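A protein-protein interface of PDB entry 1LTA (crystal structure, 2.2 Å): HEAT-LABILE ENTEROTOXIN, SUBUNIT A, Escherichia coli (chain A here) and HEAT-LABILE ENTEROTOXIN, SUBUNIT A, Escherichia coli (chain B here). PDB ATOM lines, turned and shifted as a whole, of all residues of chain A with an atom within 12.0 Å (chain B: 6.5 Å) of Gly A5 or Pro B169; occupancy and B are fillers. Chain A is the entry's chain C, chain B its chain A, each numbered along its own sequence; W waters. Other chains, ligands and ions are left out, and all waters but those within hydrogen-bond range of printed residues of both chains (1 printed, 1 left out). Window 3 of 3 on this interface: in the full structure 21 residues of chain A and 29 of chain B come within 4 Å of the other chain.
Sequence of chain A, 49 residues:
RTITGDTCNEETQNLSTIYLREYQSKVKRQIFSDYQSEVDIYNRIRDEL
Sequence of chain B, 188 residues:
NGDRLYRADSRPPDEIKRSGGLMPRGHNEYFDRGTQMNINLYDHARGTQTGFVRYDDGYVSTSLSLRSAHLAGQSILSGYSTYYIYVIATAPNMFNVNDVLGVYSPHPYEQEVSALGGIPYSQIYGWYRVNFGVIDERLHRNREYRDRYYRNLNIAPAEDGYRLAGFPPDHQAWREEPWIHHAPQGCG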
ATOM      1  N   GLY A   5      10.314 -16.644  -7.498  1.00  0.00           N
ATOM      2  CA  GLY A   5       9.267 -16.276  -6.573  1.00  0.00           C
ATOM      3  C   GLY A   5       7.985 -16.653  -7.285  1.00  0.00           C
ATOM      4  O   GLY A   5       7.783 -16.220  -8.430  1.00  0.00           O
ATOM      5  N   ASP A   6       7.214 -17.538  -6.637  1.00  0.00           N
ATOM      6  CA  ASP A   6       5.955 -18.045  -7.169  1.00  0.00           C
ATOM      7  C   ASP A   6       5.047 -16.875  -7.498  1.00  0.00           C
ATOM      8  O   ASP A   6       4.590 -16.792  -8.634  1.00  0.00           O
ATOM      9  CB  ASP A   6       5.281 -18.990  -6.121  1.00  0.00           C
ATOM     10  CG  ASP A   6       3.929 -19.669  -6.456  1.00  0.00           C
ATOM     11  OD1 ASP A   6       3.644 -19.954  -7.628  1.00  0.00           O
ATOM     12  OD2 ASP A   6       3.170 -19.951  -5.515  1.00  0.00           O
ATOM     13  N   THR A   7       4.904 -15.935  -6.566  1.00  0.00           N
ATOM     14  CA  THR A   7       4.018 -14.810  -6.735  1.00  0.00           C
ATOM     15  C   THR A   7       4.157 -14.127  -8.085  1.00  0.00           C
ATOM     16  O   THR A   7       3.112 -13.886  -8.686  1.00  0.00           O
ATOM     17  CB  THR A   7       4.287 -13.877  -5.553  1.00  0.00           C
ATOM     18  OG1 THR A   7       4.171 -14.688  -4.377  1.00  0.00           O
ATOM     19  CG2 THR A   7       3.294 -12.733  -5.456  1.00  0.00           C
ATOM     20  N   CYS A   8       5.361 -13.945  -8.639  1.00  0.00           N
ATOM     21  CA  CYS A   8       5.483 -13.385  -9.978  1.00  0.00           C
ATOM     22  C   CYS A   8       4.744 -14.229 -11.006  1.00  0.00           C
ATOM     23  O   CYS A   8       3.814 -13.791 -11.685  1.00  0.00           O
ATOM     24  CB  CYS A   8       6.922 -13.316 -10.384  1.00  0.00           C
ATOM     25  SG  CYS A   8       7.167 -12.542 -11.994  1.00  0.00           S
ATOM     26  N   ASN A   9       5.049 -15.521 -10.996  1.00  0.00           N
ATOM     27  CA  ASN A   9       4.532 -16.430 -11.994  1.00  0.00           C
ATOM     28  C   ASN A   9       3.060 -16.760 -11.902  1.00  0.00           C
ATOM     29  O   ASN A   9       2.393 -16.928 -12.932  1.00  0.00           O
ATOM     30  CB  ASN A   9       5.293 -17.726 -11.957  1.00  0.00           C
ATOM     31  CG  ASN A   9       6.737 -17.550 -12.381  1.00  0.00           C
ATOM     32  OD1 ASN A   9       7.078 -16.824 -13.327  1.00  0.00           O
ATOM     33  ND2 ASN A   9       7.639 -18.223 -11.672  1.00  0.00           N
ATOM     34  N   GLU A  10       2.524 -16.884 -10.687  1.00  0.00           N
ATOM     35  CA  GLU A  10       1.125 -17.194 -10.586  1.00  0.00           C
ATOM     36  C   GLU A  10       0.370 -15.894 -10.827  1.00  0.00           C
ATOM     37  O   GLU A  10      -0.759 -15.977 -11.319  1.00  0.00           O
ATOM     38  CB  GLU A  10       0.784 -17.831  -9.202  1.00  0.00           C
ATOM     39  CG  GLU A  10       0.763 -17.012  -7.905  1.00  0.00           C
ATOM     40  CD  GLU A  10       0.218 -17.713  -6.643  1.00  0.00           C
ATOM     41  OE1 GLU A  10      -1.004 -17.889  -6.521  1.00  0.00           O
ATOM     42  OE2 GLU A  10       1.013 -18.048  -5.756  1.00  0.00           O
ATOM     43  N   GLU A  11       0.954 -14.707 -10.569  1.00  0.00           N
ATOM     44  CA  GLU A  11       0.337 -13.441 -10.912  1.00  0.00           C
ATOM     45  C   GLU A  11       0.213 -13.357 -12.424  1.00  0.00           C
ATOM     46  O   GLU A  11      -0.887 -13.108 -12.921  1.00  0.00           O
ATOM     47  CB  GLU A  11       1.173 -12.283 -10.427  1.00  0.00           C
ATOM     48  CG  GLU A  11       0.648 -11.742  -9.127  1.00  0.00           C
ATOM     49  CD  GLU A  11      -0.652 -10.977  -9.324  1.00  0.00           C
ATOM     50  OE1 GLU A  11      -0.598  -9.822  -9.784  1.00  0.00           O
ATOM     51  OE2 GLU A  11      -1.704 -11.554  -9.020  1.00  0.00           O
ATOM     52  N   THR A  12       1.314 -13.613 -13.156  1.00  0.00           N
ATOM     53  CA  THR A  12       1.357 -13.661 -14.611  1.00  0.00           C
ATOM     54  C   THR A  12       0.256 -14.569 -15.114  1.00  0.00           C
ATOM     55  O   THR A  12      -0.619 -14.151 -15.879  1.00  0.00           O
ATOM     56  CB  THR A  12       2.763 -14.164 -15.040  1.00  0.00           C
ATOM     57  OG1 THR A  12       3.702 -13.140 -14.671  1.00  0.00           O
ATOM     58  CG2 THR A  12       2.806 -14.546 -16.522  1.00  0.00           C
ATOM     59  N   GLN A  13       0.225 -15.772 -14.578  1.00  0.00           N
ATOM     60  CA  GLN A  13      -0.819 -16.730 -14.904  1.00  0.00           C
ATOM     61  C   GLN A  13      -2.230 -16.169 -14.725  1.00  0.00           C
ATOM     62  O   GLN A  13      -3.090 -16.223 -15.606  1.00  0.00           O
ATOM     63  CB  GLN A  13      -0.620 -17.935 -14.014  1.00  0.00           C
ATOM     64  CG  GLN A  13      -1.603 -19.082 -14.143  1.00  0.00           C
ATOM     65  CD  GLN A  13      -1.612 -19.623 -15.555  1.00  0.00           C
ATOM     66  OE1 GLN A  13      -0.560 -19.794 -16.188  1.00  0.00           O
ATOM     67  NE2 GLN A  13      -2.797 -19.850 -16.092  1.00  0.00           N
ATOM     68  N   ASN A  14      -2.454 -15.562 -13.584  1.00  0.00           N
ATOM     69  CA  ASN A  14      -3.759 -15.085 -13.191  1.00  0.00           C
ATOM     70  C   ASN A  14      -4.210 -13.916 -14.042  1.00  0.00           C
ATOM     71  O   ASN A  14      -5.354 -13.859 -14.476  1.00  0.00           O
ATOM     72  CB  ASN A  14      -3.678 -14.727 -11.712  1.00  0.00           C
ATOM     73  CG  ASN A  14      -4.920 -14.033 -11.154  1.00  0.00           C
ATOM     74  OD1 ASN A  14      -5.996 -14.632 -11.006  1.00  0.00           O
ATOM     75  ND2 ASN A  14      -4.823 -12.748 -10.789  1.00  0.00           N
ATOM     76  N   GLY B 166       5.621 -12.093 -18.876  1.00  0.00           N
ATOM     77  CA  GLY B 166       5.958 -13.398 -18.339  1.00  0.00           C
ATOM     78  C   GLY B 166       7.403 -13.637 -18.002  1.00  0.00           C
ATOM     79  O   GLY B 166       7.816 -14.767 -17.735  1.00  0.00           O
ATOM     80  N   PHE B 167       8.204 -12.606 -17.996  1.00  0.00           N
ATOM     81  CA  PHE B 167       9.590 -12.763 -17.603  1.00  0.00           C
ATOM     82  C   PHE B 167       9.655 -13.367 -16.205  1.00  0.00           C
ATOM     83  O   PHE B 167       8.819 -13.092 -15.324  1.00  0.00           O
ATOM     84  CB  PHE B 167      10.338 -11.438 -17.538  1.00  0.00           C
ATOM     85  CG  PHE B 167      10.401 -10.722 -18.852  1.00  0.00           C
ATOM     86  CD1 PHE B 167      11.193 -11.198 -19.855  1.00  0.00           C
ATOM     87  CD2 PHE B 167       9.681  -9.550 -19.029  1.00  0.00           C
ATOM     88  CE1 PHE B 167      11.267 -10.479 -21.039  1.00  0.00           C
ATOM     89  CE2 PHE B 167       9.760  -8.837 -20.219  1.00  0.00           C
ATOM     90  CZ  PHE B 167      10.566  -9.307 -21.237  1.00  0.00           C
ATOM     91  N   PRO B 168      10.676 -14.195 -15.970  1.00  0.00           N
ATOM     92  CA  PRO B 168      10.923 -14.734 -14.638  1.00  0.00           C
ATOM     93  C   PRO B 168      11.080 -13.638 -13.569  1.00  0.00           C
ATOM     94  O   PRO B 168      11.499 -12.503 -13.871  1.00  0.00           O
ATOM     95  CB  PRO B 168      12.163 -15.650 -14.845  1.00  0.00           C
ATOM     96  CG  PRO B 168      12.688 -15.389 -16.234  1.00  0.00           C
ATOM     97  CD  PRO B 168      11.493 -14.851 -16.984  1.00  0.00           C
ATOM     98  N   PRO B 169      10.795 -13.951 -12.297  1.00  0.00           N
ATOM     99  CA  PRO B 169      10.870 -12.997 -11.184  1.00  0.00           C
ATOM    100  C   PRO B 169      12.206 -12.284 -11.023  1.00  0.00           C
ATOM    101  O   PRO B 169      12.229 -11.173 -10.498  1.00  0.00           O
ATOM    102  CB  PRO B 169      10.487 -13.805  -9.962  1.00  0.00           C
ATOM    103  CG  PRO B 169      10.707 -15.229 -10.417  1.00  0.00           C
ATOM    104  CD  PRO B 169      10.217 -15.211 -11.855  1.00  0.00           C
ATOM    105  N   ASP B 170      13.297 -12.903 -11.496  1.00  0.00           N
ATOM    106  CA  ASP B 170      14.642 -12.365 -11.376  1.00  0.00           C
ATOM    107  C   ASP B 170      15.125 -11.677 -12.647  1.00  0.00           C
ATOM    108  O   ASP B 170      16.245 -11.159 -12.688  1.00  0.00           O
ATOM    109  CB  ASP B 170      15.630 -13.519 -10.989  1.00  0.00           C
ATOM    110  CG  ASP B 170      15.893 -14.689 -11.963  1.00  0.00           C
ATOM    111  OD1 ASP B 170      15.365 -14.716 -13.085  1.00  0.00           O
ATOM    112  OD2 ASP B 170      16.659 -15.581 -11.578  1.00  0.00           O
ATOM    113  N   HIS B 171      14.288 -11.628 -13.685  1.00  0.00           N
ATOM    114  CA  HIS B 171      14.765 -11.157 -14.968  1.00  0.00           C
ATOM    115  C   HIS B 171      14.994  -9.665 -14.930  1.00  0.00           C
ATOM    116  O   HIS B 171      14.016  -8.991 -14.637  1.00  0.00           O
ATOM    117  CB  HIS B 171      13.744 -11.492 -16.020  1.00  0.00           C
ATOM    118  CG  HIS B 171      14.287 -11.338 -17.433  1.00  0.00           C
ATOM    119  ND1 HIS B 171      14.551 -10.222 -18.116  1.00  0.00           N
ATOM    120  CD2 HIS B 171      14.531 -12.410 -18.263  1.00  0.00           C
ATOM    121  CE1 HIS B 171      14.936 -10.585 -19.325  1.00  0.00           C
ATOM    122  NE2 HIS B 171      14.921 -11.897 -19.399  1.00  0.00           N
ATOM    123  N   TRP B 174      12.186  -6.746 -15.434  1.00  0.00           N
ATOM    124  CA  TRP B 174      11.202  -6.189 -14.495  1.00  0.00           C
ATOM    125  C   TRP B 174      11.625  -4.949 -13.735  1.00  0.00           C
ATOM    126  O   TRP B 174      10.830  -4.328 -13.033  1.00  0.00           O
ATOM    127  CB  TRP B 174      10.819  -7.200 -13.462  1.00  0.00           C
ATOM    128  CG  TRP B 174       9.997  -8.345 -13.995  1.00  0.00           C
ATOM    129  CD1 TRP B 174      10.389  -9.635 -13.773  1.00  0.00           C
ATOM    130  CD2 TRP B 174       8.839  -8.244 -14.720  1.00  0.00           C
ATOM    131  NE1 TRP B 174       9.475 -10.359 -14.353  1.00  0.00           N
ATOM    132  CE2 TRP B 174       8.543  -9.577 -14.923  1.00  0.00           C
ATOM    133  CE3 TRP B 174       8.001  -7.272 -15.235  1.00  0.00           C
ATOM    134  CZ2 TRP B 174       7.431  -9.949 -15.658  1.00  0.00           C
ATOM    135  CZ3 TRP B 174       6.886  -7.637 -15.975  1.00  0.00           C
ATOM    136  CH2 TRP B 174       6.601  -8.971 -16.180  1.00  0.00           C
ATOM    137  N   ARG B 175      12.923  -4.648 -13.868  1.00  0.00           N
ATOM    138  CA  ARG B 175      13.658  -3.548 -13.228  1.00  0.00           C
ATOM    139  C   ARG B 175      13.904  -2.376 -14.178  1.00  0.00           C
ATOM    140  O   ARG B 175      14.464  -1.349 -13.779  1.00  0.00           O
ATOM    141  CB  ARG B 175      15.025  -4.042 -12.725  1.00  0.00           C
ATOM    142  CG  ARG B 175      15.057  -4.973 -11.498  1.00  0.00           C
ATOM    143  CD  ARG B 175      15.746  -6.370 -11.698  1.00  0.00           C
ATOM    144  NE  ARG B 175      14.828  -7.397 -12.220  1.00  0.00           N
ATOM    145  CZ  ARG B 175      14.148  -8.272 -11.447  1.00  0.00           C
ATOM    146  NH1 ARG B 175      14.260  -8.298 -10.110  1.00  0.00           N
ATOM    147  NH2 ARG B 175      13.234  -9.067 -12.016  1.00  0.00           N
ATOM    148  N   GLY B 186       5.177  -9.417  -7.248  1.00  0.00           N
ATOM    149  CA  GLY B 186       6.158 -10.452  -7.009  1.00  0.00           C
ATOM    150  C   GLY B 186       7.182 -10.567  -8.120  1.00  0.00           C
ATOM    151  O   GLY B 186       8.008 -11.480  -8.094  1.00  0.00           O
ATOM    152  N   CYS B 187       7.123  -9.698  -9.124  1.00  0.00           N
ATOM    153  CA  CYS B 187       8.089  -9.670 -10.217  1.00  0.00           C
ATOM    154  C   CYS B 187       8.946  -8.426  -9.982  1.00  0.00           C
ATOM    155  O   CYS B 187       8.330  -7.352  -9.920  1.00  0.00           O
ATOM    156  CB  CYS B 187       7.372  -9.536 -11.577  1.00  0.00           C
ATOM    157  SG  CYS B 187       6.133 -10.797 -11.935  1.00  0.00           S
ATOM    158  N   GLY B 188      10.289  -8.503  -9.851  1.00  0.00           N
ATOM    159  CA  GLY B 188      11.127  -7.330  -9.593  1.00  0.00           C
ATOM    160  C   GLY B 188      11.946  -7.448  -8.302  1.00  0.00           C
ATOM    161  O   GLY B 188      12.047  -6.472  -7.548  1.00  0.00           O
HETATM  162  O   HOH W   1       4.014 -11.109 -16.664  1.00  0.00           O
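N of Gly A5 touches CG of Pro B169 (3.3 Å). CA of Gly B186 touches CG2 of Thr A7, at 3.98 Å. Pro B169 touches Cys A8. Cys A8 touches Trp B174 (SG to NE1, 3.96 Å). Cys A8 touches Gly B186. OD1 of Asn A9 touches CD of Pro B169, 3.8 Å away. Thr A12 touches Gly B166.
Water W1 lies within hydrogen-bond range of the side-chain hydroxyl of Thr A12 (2.9 Å) and the backbone NH of Gly B166 (2.9 Å).
Gly A5 touches just one residue of chain B: Pro B169 (3.3 Å). Pro B169 touches three residues of chain A. No residue of chain A comes within 4 Å of Pro B168. No residue of chain A comes within 4 Å of Asp B170. Cys B187 touches one residue of chain A. Printed residues of chain A within 4 Å of Trp B174: Cys A8 (3.96 Å). Printed residues of chain A within 4 Å of Phe B167: Cys A8 (3.8 Å). Printed residues of chain A within 4 Å of Gly B166: Thr A12. Printed residues of chain B within 4 Å of Asn A9: Pro B169 (3.8 Å). The nearest residue of chain A that does not touch Pro B169 is Asp A6 (5.6 Å).
The side-chain sulfur of Cys A8 is disulfide-bonded to the side-chain sulfur of Cys B187, 2.0 Å away. SG of Cys A8 lies close to O of Phe B167, 3.8 Å away.
Printed residues of chain A that touch a printed residue of chain B: Gly A5, Thr A7, Cys A8, Asn A9 and Thr A12. Of the 11 printed residues of chain B, 6 touch a printed residue of chain A. Printed residues of chain B that touch a printed residue of chain A: Gly B166, Phe B167, Pro B169, Trp B174, Gly B186 and Cys B187. Hydrophobic or aromatic side chains of chain B within 4 Å of the printed part of chain A: Pro B169 and Trp B174.
The backbone carbonyl oxygen (O) of Pro B169 is in hydrogen-bond range of the backbone NH (N) of Gly B188. The guanidinium group (NH2) of Arg B175 is in hydrogen-bond range of the backbone carbonyl oxygen (O) of Pro B169, 2.8 Å away. The indole nitrogen (NE1) of Trp B174 sits at hydrogen-bond distance from the backbone carbonyl oxygen (O) of Phe B167, 3.0 Å away. NE1 of Trp B174 sits at hydrogen-bond distance from O of Pro B168, at 3.0 Å. The backbone carbonyl oxygen of Cys A8 lies within hydrogen-bond range of the side-chain hydroxyl of Thr A12, 3.1 Å away.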
